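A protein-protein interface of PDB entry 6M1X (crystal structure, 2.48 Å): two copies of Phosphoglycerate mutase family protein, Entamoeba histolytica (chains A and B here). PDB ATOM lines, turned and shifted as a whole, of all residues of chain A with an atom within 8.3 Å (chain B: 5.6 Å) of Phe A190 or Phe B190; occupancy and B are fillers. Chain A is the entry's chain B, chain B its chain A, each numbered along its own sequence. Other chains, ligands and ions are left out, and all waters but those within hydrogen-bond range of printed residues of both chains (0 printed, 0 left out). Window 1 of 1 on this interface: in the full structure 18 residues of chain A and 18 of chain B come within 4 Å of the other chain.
N of Gln B169 lies within hydrogen-bond range of O of Leu A187 (3.0 Å). The backbone carbonyl oxygen (O) of Lys A167 lies within hydrogen-bond range of the backbone NH (N) of Leu B187 (2.9 Å). The backbone NH (N) of Gln A169 lies within hydrogen-bond range of the backbone carbonyl oxygen (O) of Leu B187, at 3.0 Å. The backbone carbonyl oxygen (O) of Thr B188 is in hydrogen-bond range of the side-chain amide nitrogen (ND2) of Asn A191 (2.8 Å). The backbone carbonyl oxygen of Phe A190 is in hydrogen-bond range of the backbone NH of Phe B190 (3.1 Å). The side-chain amide nitrogen of Asn B191 lies within hydrogen-bond range of the backbone carbonyl oxygen of Thr A188.
O of Ile B175 is in hydrogen-bond range of N of Asn B191 (2.9 Å). The backbone NH of Asn B191 lies within hydrogen-bond range of the side-chain hydroxyl of Thr B176 (3.4 Å). OG1 of Thr B177 sits at hydrogen-bond distance from OG1 of Thr B188, at 2.6 Å. O of Ser B189 sits at hydrogen-bond distance from N of Thr B177 (3.1 Å). O of Ile A175 sits at hydrogen-bond distance from N of Asn A191 (2.6 Å). The side-chain hydroxyl (OG1) of Thr A176 is in hydrogen-bond range of the backbone NH (N) of Asn A191 (3.1 Å).
Among the printed residues, merely in contact across the chains: Phe A168 with Leu B187 (3.7 Å), Gln A169 with Thr B188 (3.9 Å), Val A186 with Phe B168 (3.9 Å), Leu A187 with Phe B168 (3.6 Å), Leu A187 with Phe B190 (3.6 Å), Thr A188 with Gln B169 (3.8 Å), Ser A189 with Phe B190 (3.5 Å), Phe A190 with Leu B187 (3.5 Å), Phe A190 with Ser B189 (3.3 Å) and Ser A192 with Ser B192 (3.6 Å).
Phe A190 touches just these residues of chain B: Leu B187 (3.5 Å), Ser B189 (3.3 Å) and Phe B190 (3.1 Å). Of the printed residues of chain A, Phe B190 touches Leu A187, Ser A189 and Phe A190. Ser B189 touches just one residue of chain A: Phe A190 (3.3 Å). Of the printed residues of chain A, Leu B187 touches Lys A167 (2.9 Å), Phe A168 (3.7 Å), Gln A169 (3.0 Å) and Phe A190 (3.5 Å). Of the printed residues of chain B, Lys A167 touches Leu B187 (2.9 Å). Printed residues of chain A within 4 Å of Phe B168: Val A186 and Leu A187. Printed residues of chain A within 4 Å of Gln B169: Leu A187 (3.0 Å) and Thr A188 (3.8 Å). Thr A193 touches none of the printed residues of chain B. The nearest residue of chain B that does not touch Phe A190 is Thr B188 (4.1 Å). The nearest printed residue of chain B that does not touch Gln A169 is Ser B189 (5.1 Å).
Hydrophobic or aromatic side chains of chain B within 4 Å of the printed part of chain A: Phe B168, Leu B187 and Phe B190. Along chain B the printed residues that touch a printed residue of chain A span positions 168 to 192. Of the 25 printed residues of chain A, 10 touch a printed residue of chain B. Along chain A the printed residues that touch a printed residue of chain B span positions 167 to 192. Among the printed residues, 16 pairs touch across the chains.
Phe A168 touches Leu B187, and with the chains exchanged Leu A187 touches Phe B168. Gln A169 touches Leu B187, and with the chains exchanged Leu A187 touches Gln B169. Gln A169 touches Thr B188, and with the chains exchanged Thr A188 touches Gln B169. Thr A188 touches Asn B191, and with the chains exchanged Asn A191 touches Thr B188. 13 positions are printed for both chains. Of the 16 pairs that touch across the chains among the printed residues, 14 have their exchanged pair printed and touching as well.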
ATOM      1  N   LEU A   6       0.458  23.498  18.245  1.00  0.00           N
ATOM      2  CA  LEU A   6       0.506  22.517  17.195  1.00  0.00           C
ATOM      3  C   LEU A   6       0.238  21.177  17.803  1.00  0.00           C
ATOM      4  O   LEU A   6       0.887  20.808  18.747  1.00  0.00           O
ATOM      5  CB  LEU A   6       1.857  22.530  16.558  1.00  0.00           C
ATOM      6  CG  LEU A   6       2.305  23.810  15.914  1.00  0.00           C
ATOM      7  CD1 LEU A   6       3.601  23.493  15.159  1.00  0.00           C
ATOM      8  CD2 LEU A   6       1.245  24.359  14.980  1.00  0.00           C
ATOM      9  N   GLY A 147       2.714  14.258  11.860  1.00  0.00           N
ATOM     10  CA  GLY A 147       4.048  14.148  12.467  1.00  0.00           C
ATOM     11  C   GLY A 147       5.207  14.864  11.708  1.00  0.00           C
ATOM     12  O   GLY A 147       5.885  15.765  12.222  1.00  0.00           O
ATOM     13  N   ILE A 150       4.573  18.915  11.372  1.00  0.00           N
ATOM     14  CA  ILE A 150       4.817  19.665  12.592  1.00  0.00           C
ATOM     15  C   ILE A 150       6.326  19.743  12.900  1.00  0.00           C
ATOM     16  O   ILE A 150       6.821  20.821  13.251  1.00  0.00           O
ATOM     17  CB  ILE A 150       4.026  19.035  13.737  1.00  0.00           C
ATOM     18  CG1 ILE A 150       2.533  19.242  13.476  1.00  0.00           C
ATOM     19  CG2 ILE A 150       4.393  19.670  15.058  1.00  0.00           C
ATOM     20  CD1 ILE A 150       1.574  18.671  14.546  1.00  0.00           C
ATOM     21  N   LYS A 151       7.032  18.621  12.767  1.00  0.00           N
ATOM     22  CA  LYS A 151       8.465  18.549  13.071  1.00  0.00           C
ATOM     23  C   LYS A 151       9.283  19.503  12.195  1.00  0.00           C
ATOM     24  O   LYS A 151      10.135  20.231  12.696  1.00  0.00           O
ATOM     25  CB  LYS A 151       8.974  17.104  12.938  1.00  0.00           C
ATOM     26  CG  LYS A 151       8.881  16.281  14.229  1.00  0.00           C
ATOM     27  CD  LYS A 151       8.842  14.754  14.035  1.00  0.00           C
ATOM     28  CE  LYS A 151      10.220  14.126  13.875  1.00  0.00           C
ATOM     29  NZ  LYS A 151      10.081  12.664  13.567  1.00  0.00           N
ATOM     30  N   ILE A 154       8.766  23.049  13.250  1.00  0.00           N
ATOM     31  CA  ILE A 154       9.631  23.387  14.374  1.00  0.00           C
ATOM     32  C   ILE A 154      10.992  23.805  13.830  1.00  0.00           C
ATOM     33  O   ILE A 154      11.475  24.897  14.153  1.00  0.00           O
ATOM     34  CB  ILE A 154       9.754  22.212  15.346  1.00  0.00           C
ATOM     35  CG1 ILE A 154       8.457  22.057  16.112  1.00  0.00           C
ATOM     36  CG2 ILE A 154      10.923  22.403  16.319  1.00  0.00           C
ATOM     37  CD1 ILE A 154       8.205  20.653  16.621  1.00  0.00           C
ATOM     38  N   LEU A 158      12.256  27.572  14.532  1.00  0.00           N
ATOM     39  CA  LEU A 158      13.455  27.780  15.355  1.00  0.00           C
ATOM     40  C   LEU A 158      14.753  27.783  14.545  1.00  0.00           C
ATOM     41  O   LEU A 158      15.862  27.792  15.112  1.00  0.00           O
ATOM     42  CB  LEU A 158      13.504  26.713  16.446  1.00  0.00           C
ATOM     43  CG  LEU A 158      12.259  26.715  17.314  1.00  0.00           C
ATOM     44  CD1 LEU A 158      12.447  25.768  18.486  1.00  0.00           C
ATOM     45  CD2 LEU A 158      11.918  28.102  17.831  1.00  0.00           C
ATOM     46  N   TYR A 165      15.768  17.154  12.845  1.00  0.00           N
ATOM     47  CA  TYR A 165      14.515  16.423  12.672  1.00  0.00           C
ATOM     48  C   TYR A 165      14.462  15.044  13.348  1.00  0.00           C
ATOM     49  O   TYR A 165      13.402  14.623  13.822  1.00  0.00           O
ATOM     50  CB  TYR A 165      14.244  16.258  11.176  1.00  0.00           C
ATOM     51  CG  TYR A 165      12.983  15.510  10.802  1.00  0.00           C
ATOM     52  CD1 TYR A 165      12.914  14.111  10.887  1.00  0.00           C
ATOM     53  CD2 TYR A 165      11.886  16.190  10.307  1.00  0.00           C
ATOM     54  CE1 TYR A 165      11.775  13.422  10.497  1.00  0.00           C
ATOM     55  CE2 TYR A 165      10.744  15.520   9.904  1.00  0.00           C
ATOM     56  CZ  TYR A 165      10.686  14.135  10.001  1.00  0.00           C
ATOM     57  OH  TYR A 165       9.519  13.512   9.625  1.00  0.00           O
ATOM     58  N   LYS A 167      16.243  14.097  15.943  1.00  0.00           N
ATOM     59  CA  LYS A 167      16.416  14.303  17.398  1.00  0.00           C
ATOM     60  C   LYS A 167      15.119  14.727  18.094  1.00  0.00           C
ATOM     61  O   LYS A 167      15.099  14.980  19.297  1.00  0.00           O
ATOM     62  CB  LYS A 167      17.492  15.365  17.665  1.00  0.00           C
ATOM     63  CG  LYS A 167      18.758  15.158  16.852  1.00  0.00           C
ATOM     64  CD  LYS A 167      19.974  15.754  17.522  1.00  0.00           C
ATOM     65  CE  LYS A 167      21.136  15.866  16.538  1.00  0.00           C
ATOM     66  NZ  LYS A 167      22.401  15.392  17.125  1.00  0.00           N
ATOM     67  N   PHE A 168      14.047  14.828  17.329  1.00  0.00           N
ATOM     68  CA  PHE A 168      12.762  15.124  17.888  1.00  0.00           C
ATOM     69  C   PHE A 168      11.911  13.917  17.674  1.00  0.00           C
ATOM     70  O   PHE A 168      12.022  13.281  16.649  1.00  0.00           O
ATOM     71  CB  PHE A 168      12.115  16.284  17.166  1.00  0.00           C
ATOM     72  CG  PHE A 168      12.560  17.616  17.636  1.00  0.00           C
ATOM     73  CD1 PHE A 168      13.609  18.279  17.005  1.00  0.00           C
ATOM     74  CD2 PHE A 168      11.897  18.234  18.680  1.00  0.00           C
ATOM     75  CE1 PHE A 168      14.021  19.514  17.419  1.00  0.00           C
ATOM     76  CE2 PHE A 168      12.290  19.474  19.098  1.00  0.00           C
ATOM     77  CZ  PHE A 168      13.364  20.122  18.468  1.00  0.00           C
ATOM     78  N   GLN A 169      11.056  13.635  18.655  1.00  0.00           N
ATOM     79  CA  GLN A 169      10.092  12.597  18.530  1.00  0.00           C
ATOM     80  C   GLN A 169       8.752  13.130  19.000  1.00  0.00           C
ATOM     81  O   GLN A 169       8.608  13.523  20.150  1.00  0.00           O
ATOM     82  CB  GLN A 169      10.456  11.387  19.340  1.00  0.00           C
ATOM     83  CG  GLN A 169       9.307  10.415  19.359  1.00  0.00           C
ATOM     84  CD  GLN A 169       9.629   9.192  20.122  1.00  0.00           C
ATOM     85  OE1 GLN A 169      10.525   8.466  19.732  1.00  0.00           O
ATOM     86  NE2 GLN A 169       8.901   8.938  21.226  1.00  0.00           N
ATOM     87  N   LEU A 170       7.770  13.062  18.093  1.00  0.00           N
ATOM     88  CA  LEU A 170       6.427  13.538  18.331  1.00  0.00           C
ATOM     89  C   LEU A 170       5.431  12.419  18.366  1.00  0.00           C
ATOM     90  O   LEU A 170       5.445  11.570  17.490  1.00  0.00           O
ATOM     91  CB  LEU A 170       6.090  14.474  17.193  1.00  0.00           C
ATOM     92  CG  LEU A 170       4.855  15.354  17.281  1.00  0.00           C
ATOM     93  CD1 LEU A 170       4.497  15.833  18.674  1.00  0.00           C
ATOM     94  CD2 LEU A 170       5.063  16.512  16.307  1.00  0.00           C
ATOM     95  N   GLY A 171       4.567  12.436  19.383  1.00  0.00           N
ATOM     96  CA  GLY A 171       3.518  11.409  19.620  1.00  0.00           C
ATOM     97  C   GLY A 171       2.110  11.858  19.258  1.00  0.00           C
ATOM     98  O   GLY A 171       1.862  13.031  19.069  1.00  0.00           O
ATOM     99  N   GLY A 174       0.397  14.782  20.748  1.00  0.00           N
ATOM    100  CA  GLY A 174       1.468  15.576  21.287  1.00  0.00           C
ATOM    101  C   GLY A 174       1.189  17.059  21.048  1.00  0.00           C
ATOM    102  O   GLY A 174       0.855  17.454  19.949  1.00  0.00           O
ATOM    103  N   ILE A 175       1.332  17.879  22.078  1.00  0.00           N
ATOM    104  CA  ILE A 175       1.157  19.329  21.967  1.00  0.00           C
ATOM    105  C   ILE A 175       2.503  20.001  21.855  1.00  0.00           C
ATOM    106  O   ILE A 175       3.473  19.535  22.424  1.00  0.00           O
ATOM    107  CB  ILE A 175       0.440  19.842  23.179  1.00  0.00           C
ATOM    108  CG1 ILE A 175      -0.830  19.017  23.374  1.00  0.00           C
ATOM    109  CG2 ILE A 175       0.140  21.330  23.037  1.00  0.00           C
ATOM    110  CD1 ILE A 175      -1.717  19.497  24.505  1.00  0.00           C
ATOM    111  N   THR A 176       2.562  21.086  21.108  1.00  0.00           N
ATOM    112  CA  THR A 176       3.789  21.852  20.908  1.00  0.00           C
ATOM    113  C   THR A 176       3.395  23.322  20.784  1.00  0.00           C
ATOM    114  O   THR A 176       2.652  23.665  19.895  1.00  0.00           O
ATOM    115  CB  THR A 176       4.564  21.364  19.683  1.00  0.00           C
ATOM    116  OG1 THR A 176       5.200  20.126  19.980  1.00  0.00           O
ATOM    117  CG2 THR A 176       5.664  22.329  19.264  1.00  0.00           C
ATOM    118  N   THR A 177       3.872  24.173  21.689  1.00  0.00           N
ATOM    119  CA  THR A 177       3.510  25.572  21.662  1.00  0.00           C
ATOM    120  C   THR A 177       4.695  26.530  21.357  1.00  0.00           C
ATOM    121  O   THR A 177       5.858  26.220  21.556  1.00  0.00           O
ATOM    122  CB  THR A 177       2.774  26.002  22.944  1.00  0.00           C
ATOM    123  OG1 THR A 177       3.718  26.235  23.947  1.00  0.00           O
ATOM    124  CG2 THR A 177       1.834  24.921  23.476  1.00  0.00           C
ATOM    125  N   PHE A 178       4.355  27.696  20.842  1.00  0.00           N
ATOM    126  CA  PHE A 178       5.295  28.744  20.555  1.00  0.00           C
ATOM    127  C   PHE A 178       4.681  30.063  21.060  1.00  0.00           C
ATOM    128  O   PHE A 178       3.461  30.181  21.159  1.00  0.00           O
ATOM    129  CB  PHE A 178       5.533  28.872  19.067  1.00  0.00           C
ATOM    130  CG  PHE A 178       6.323  27.784  18.495  1.00  0.00           C
ATOM    131  CD1 PHE A 178       5.693  26.620  18.049  1.00  0.00           C
ATOM    132  CD2 PHE A 178       7.697  27.901  18.387  1.00  0.00           C
ATOM    133  CE1 PHE A 178       6.436  25.582  17.500  1.00  0.00           C
ATOM    134  CE2 PHE A 178       8.448  26.855  17.835  1.00  0.00           C
ATOM    135  CZ  PHE A 178       7.827  25.696  17.388  1.00  0.00           C
ATOM    136  N   VAL A 186       9.474  31.409  20.048  1.00  0.00           N
ATOM    137  CA  VAL A 186      10.192  30.766  21.135  1.00  0.00           C
ATOM    138  C   VAL A 186       9.379  29.517  21.509  1.00  0.00           C
ATOM    139  O   VAL A 186       8.178  29.636  21.832  1.00  0.00           O
ATOM    140  CB  VAL A 186      10.280  31.707  22.348  1.00  0.00           C
ATOM    141  CG1 VAL A 186      10.989  31.042  23.491  1.00  0.00           C
ATOM    142  CG2 VAL A 186      11.078  32.941  22.004  1.00  0.00           C
ATOM    143  N   LEU A 187       9.997  28.330  21.459  1.00  0.00           N
ATOM    144  CA  LEU A 187       9.316  27.094  21.854  1.00  0.00           C
ATOM    145  C   LEU A 187       9.057  27.061  23.351  1.00  0.00           C
ATOM    146  O   LEU A 187       9.975  27.234  24.129  1.00  0.00           O
ATOM    147  CB  LEU A 187      10.139  25.887  21.417  1.00  0.00           C
ATOM    148  CG  LEU A 187       9.634  24.501  21.837  1.00  0.00           C
ATOM    149  CD1 LEU A 187       8.512  24.090  20.941  1.00  0.00           C
ATOM    150  CD2 LEU A 187      10.701  23.455  21.750  1.00  0.00           C
ATOM    151  N   THR A 188       7.817  26.874  23.756  1.00  0.00           N
ATOM    152  CA  THR A 188       7.456  26.775  25.179  1.00  0.00           C
ATOM    153  C   THR A 188       6.848  25.432  25.580  1.00  0.00           C
ATOM    154  O   THR A 188       6.638  25.178  26.764  1.00  0.00           O
ATOM    155  CB  THR A 188       6.485  27.883  25.613  1.00  0.00           C
ATOM    156  OG1 THR A 188       5.214  27.652  25.078  1.00  0.00           O
ATOM    157  CG2 THR A 188       6.920  29.250  25.159  1.00  0.00           C
ATOM    158  N   SER A 189       6.581  24.568  24.610  1.00  0.00           N
ATOM    159  CA  SER A 189       6.338  23.165  24.895  1.00  0.00           C
ATOM    160  C   SER A 189       6.599  22.368  23.643  1.00  0.00           C
ATOM    161  O   SER A 189       6.441  22.876  22.566  1.00  0.00           O
ATOM    162  CB  SER A 189       4.915  22.909  25.427  1.00  0.00           C
ATOM    163  OG  SER A 189       4.006  22.755  24.370  1.00  0.00           O
ATOM    164  N   PHE A 190       6.966  21.109  23.827  1.00  0.00           N
ATOM    165  CA  PHE A 190       7.075  20.131  22.749  1.00  0.00           C
ATOM    166  C   PHE A 190       6.546  18.772  23.217  1.00  0.00           C
ATOM    167  O   PHE A 190       6.885  18.281  24.287  1.00  0.00           O
ATOM    168  CB  PHE A 190       8.509  20.003  22.226  1.00  0.00           C
ATOM    169  CG  PHE A 190       8.692  18.842  21.293  1.00  0.00           C
ATOM    170  CD1 PHE A 190       8.303  18.925  19.986  1.00  0.00           C
ATOM    171  CD2 PHE A 190       9.240  17.646  21.740  1.00  0.00           C
ATOM    172  CE1 PHE A 190       8.466  17.825  19.120  1.00  0.00           C
ATOM    173  CE2 PHE A 190       9.388  16.547  20.904  1.00  0.00           C
ATOM    174  CZ  PHE A 190       9.006  16.629  19.579  1.00  0.00           C
ATOM    175  N   ASN A 191       5.704  18.187  22.393  1.00  0.00           N
ATOM    176  CA  ASN A 191       5.151  16.870  22.640  1.00  0.00           C
ATOM    177  C   ASN A 191       4.566  16.625  24.044  1.00  0.00           C
ATOM    178  O   ASN A 191       4.653  15.549  24.544  1.00  0.00           O
ATOM    179  CB  ASN A 191       6.176  15.785  22.265  1.00  0.00           C
ATOM    180  CG  ASN A 191       5.525  14.424  22.001  1.00  0.00           C
ATOM    181  OD1 ASN A 191       4.359  14.342  21.602  1.00  0.00           O
ATOM    182  ND2 ASN A 191       6.261  13.352  22.254  1.00  0.00           N
ATOM    183  N   SER A 192       3.949  17.612  24.655  1.00  0.00           N
ATOM    184  CA  SER A 192       3.250  17.329  25.908  1.00  0.00           C
ATOM    185  C   SER A 192       2.150  16.309  25.756  1.00  0.00           C
ATOM    186  O   SER A 192       1.286  16.482  24.921  1.00  0.00           O
ATOM    187  CB  SER A 192       2.664  18.580  26.476  1.00  0.00           C
ATOM    188  OG  SER A 192       3.647  19.578  26.297  1.00  0.00           O
ATOM    189  N   THR A 193       2.197  15.270  26.585  1.00  0.00           N
ATOM    190  CA  THR A 193       1.298  14.126  26.468  1.00  0.00           C
ATOM    191  C   THR A 193       0.639  13.715  27.806  1.00  0.00           C
ATOM    192  O   THR A 193       0.169  12.575  27.967  1.00  0.00           O
ATOM    193  CB  THR A 193       2.017  12.909  25.867  1.00  0.00           C
ATOM    194  OG1 THR A 193       3.303  12.755  26.458  1.00  0.00           O
ATOM    195  CG2 THR A 193       2.175  13.058  24.379  1.00  0.00           C
ATOM    196  N   ILE B 154      19.985  20.588  27.175  1.00  0.00           N
ATOM    197  CA  ILE B 154      19.261  20.270  25.951  1.00  0.00           C
ATOM    198  C   ILE B 154      20.140  20.623  24.779  1.00  0.00           C
ATOM    199  O   ILE B 154      20.251  19.854  23.858  1.00  0.00           O
ATOM    200  CB  ILE B 154      17.897  20.986  25.852  1.00  0.00           C
ATOM    201  CG1 ILE B 154      16.953  20.596  27.008  1.00  0.00           C
ATOM    202  CG2 ILE B 154      17.209  20.661  24.525  1.00  0.00           C
ATOM    203  CD1 ILE B 154      16.005  21.736  27.413  1.00  0.00           C
ATOM    204  N   PHE B 168      14.199  28.651  23.740  1.00  0.00           N
ATOM    205  CA  PHE B 168      13.500  27.798  24.666  1.00  0.00           C
ATOM    206  C   PHE B 168      13.001  28.611  25.827  1.00  0.00           C
ATOM    207  O   PHE B 168      13.614  29.574  26.197  1.00  0.00           O
ATOM    208  CB  PHE B 168      14.416  26.728  25.149  1.00  0.00           C
ATOM    209  CG  PHE B 168      14.704  25.701  24.137  1.00  0.00           C
ATOM    210  CD1 PHE B 168      15.725  25.875  23.230  1.00  0.00           C
ATOM    211  CD2 PHE B 168      13.964  24.518  24.110  1.00  0.00           C
ATOM    212  CE1 PHE B 168      15.996  24.887  22.284  1.00  0.00           C
ATOM    213  CE2 PHE B 168      14.224  23.526  23.177  1.00  0.00           C
ATOM    214  CZ  PHE B 168      15.252  23.707  22.264  1.00  0.00           C
ATOM    215  N   GLN B 169      11.821  28.280  26.320  1.00  0.00           N
ATOM    216  CA  GLN B 169      11.328  28.857  27.573  1.00  0.00           C
ATOM    217  C   GLN B 169      10.801  27.747  28.453  1.00  0.00           C
ATOM    218  O   GLN B 169       9.941  27.008  28.068  1.00  0.00           O
ATOM    219  CB  GLN B 169      10.247  29.856  27.356  1.00  0.00           C
ATOM    220  CG  GLN B 169       9.960  30.706  28.581  1.00  0.00           C
ATOM    221  CD  GLN B 169       8.960  31.789  28.210  1.00  0.00           C
ATOM    222  OE1 GLN B 169       9.354  32.884  27.730  1.00  0.00           O
ATOM    223  NE2 GLN B 169       7.650  31.471  28.359  1.00  0.00           N
ATOM    224  N   LEU B 170      11.393  27.654  29.623  1.00  0.00           N
ATOM    225  CA  LEU B 170      11.267  26.512  30.472  1.00  0.00           C
ATOM    226  C   LEU B 170      10.709  27.031  31.765  1.00  0.00           C
ATOM    227  O   LEU B 170      11.389  27.702  32.493  1.00  0.00           O
ATOM    228  CB  LEU B 170      12.617  25.884  30.659  1.00  0.00           C
ATOM    229  CG  LEU B 170      12.778  24.696  31.583  1.00  0.00           C
ATOM    230  CD1 LEU B 170      11.756  23.593  31.406  1.00  0.00           C
ATOM    231  CD2 LEU B 170      14.177  24.193  31.259  1.00  0.00           C
ATOM    232  N   ILE B 175       8.626  19.631  32.669  1.00  0.00           N
ATOM    233  CA  ILE B 175       9.301  18.362  32.409  1.00  0.00           C
ATOM    234  C   ILE B 175       9.927  18.317  30.996  1.00  0.00           C
ATOM    235  O   ILE B 175       9.330  18.756  30.024  1.00  0.00           O
ATOM    236  CB  ILE B 175       8.312  17.208  32.538  1.00  0.00           C
ATOM    237  CG1 ILE B 175       7.549  17.287  33.876  1.00  0.00           C
ATOM    238  CG2 ILE B 175       9.060  15.917  32.364  1.00  0.00           C
ATOM    239  CD1 ILE B 175       6.501  16.229  34.056  1.00  0.00           C
ATOM    240  N   THR B 176      11.126  17.760  30.912  1.00  0.00           N
ATOM    241  CA  THR B 176      11.813  17.578  29.676  1.00  0.00           C
ATOM    242  C   THR B 176      12.361  16.172  29.757  1.00  0.00           C
ATOM    243  O   THR B 176      13.044  15.851  30.706  1.00  0.00           O
ATOM    244  CB  THR B 176      12.936  18.586  29.492  1.00  0.00           C
ATOM    245  OG1 THR B 176      12.391  19.895  29.400  1.00  0.00           O
ATOM    246  CG2 THR B 176      13.733  18.302  28.218  1.00  0.00           C
ATOM    247  N   THR B 177      12.087  15.345  28.741  1.00  0.00           N
ATOM    248  CA  THR B 177      12.505  13.947  28.717  1.00  0.00           C
ATOM    249  C   THR B 177      13.283  13.601  27.432  1.00  0.00           C
ATOM    250  O   THR B 177      13.006  14.108  26.335  1.00  0.00           O
ATOM    251  CB  THR B 177      11.283  13.015  28.893  1.00  0.00           C
ATOM    252  OG1 THR B 177      10.588  12.918  27.669  1.00  0.00           O
ATOM    253  CG2 THR B 177      10.278  13.584  29.863  1.00  0.00           C
ATOM    254  N   LEU B 187      14.929  13.864  21.920  1.00  0.00           N
ATOM    255  CA  LEU B 187      14.006  14.639  22.731  1.00  0.00           C
ATOM    256  C   LEU B 187      12.573  14.149  22.520  1.00  0.00           C
ATOM    257  O   LEU B 187      12.060  14.284  21.418  1.00  0.00           O
ATOM    258  CB  LEU B 187      14.141  16.129  22.384  1.00  0.00           C
ATOM    259  CG  LEU B 187      13.266  17.042  23.239  1.00  0.00           C
ATOM    260  CD1 LEU B 187      13.852  17.226  24.604  1.00  0.00           C
ATOM    261  CD2 LEU B 187      13.122  18.382  22.572  1.00  0.00           C
ATOM    262  N   THR B 188      11.956  13.578  23.551  1.00  0.00           N
ATOM    263  CA  THR B 188      10.564  13.137  23.454  1.00  0.00           C
ATOM    264  C   THR B 188       9.586  14.088  24.120  1.00  0.00           C
ATOM    265  O   THR B 188       8.396  13.859  24.034  1.00  0.00           O
ATOM    266  CB  THR B 188      10.348  11.691  24.000  1.00  0.00           C
ATOM    267  OG1 THR B 188      10.343  11.667  25.417  1.00  0.00           O
ATOM    268  CG2 THR B 188      11.423  10.789  23.513  1.00  0.00           C
ATOM    269  N   SER B 189      10.076  15.116  24.818  1.00  0.00           N
ATOM    270  CA  SER B 189       9.205  16.153  25.376  1.00  0.00           C
ATOM    271  C   SER B 189      10.024  17.288  25.972  1.00  0.00           C
ATOM    272  O   SER B 189      11.162  17.078  26.326  1.00  0.00           O
ATOM    273  CB  SER B 189       8.236  15.598  26.427  1.00  0.00           C
ATOM    274  OG  SER B 189       8.848  15.512  27.687  1.00  0.00           O
ATOM    275  N   PHE B 190       9.431  18.481  26.043  1.00  0.00           N
ATOM    276  CA  PHE B 190      10.074  19.665  26.607  1.00  0.00           C
ATOM    277  C   PHE B 190       9.050  20.550  27.276  1.00  0.00           C
ATOM    278  O   PHE B 190       7.965  20.678  26.794  1.00  0.00           O
ATOM    279  CB  PHE B 190      10.816  20.493  25.547  1.00  0.00           C
ATOM    280  CG  PHE B 190      11.154  21.903  26.019  1.00  0.00           C
ATOM    281  CD1 PHE B 190      12.224  22.145  26.812  1.00  0.00           C
ATOM    282  CD2 PHE B 190      10.357  22.976  25.684  1.00  0.00           C
ATOM    283  CE1 PHE B 190      12.492  23.420  27.260  1.00  0.00           C
ATOM    284  CE2 PHE B 190      10.638  24.265  26.107  1.00  0.00           C
ATOM    285  CZ  PHE B 190      11.696  24.477  26.905  1.00  0.00           C
ATOM    286  N   ASN B 191       9.419  21.142  28.400  1.00  0.00           N
ATOM    287  CA  ASN B 191       8.551  21.954  29.239  1.00  0.00           C
ATOM    288  C   ASN B 191       7.061  21.588  29.352  1.00  0.00           C
ATOM    289  O   ASN B 191       6.179  22.447  29.319  1.00  0.00           O
ATOM    290  CB  ASN B 191       8.697  23.403  28.832  1.00  0.00           C
ATOM    291  CG  ASN B 191       8.216  24.368  29.907  1.00  0.00           C
ATOM    292  OD1 ASN B 191       8.527  24.244  31.103  1.00  0.00           O
ATOM    293  ND2 ASN B 191       7.451  25.343  29.478  1.00  0.00           N
ATOM    294  N   SER B 192       6.784  20.322  29.521  1.00  0.00           N
ATOM    295  CA  SER B 192       5.420  19.897  29.773  1.00  0.00           C
ATOM    296  C   SER B 192       4.987  20.380  31.133  1.00  0.00           C
ATOM    297  O   SER B 192       5.635  20.056  32.131  1.00  0.00           O
ATOM    298  CB  SER B 192       5.297  18.379  29.689  1.00  0.00           C
ATOM    299  OG  SER B 192       5.946  17.916  28.541  1.00  0.00           O
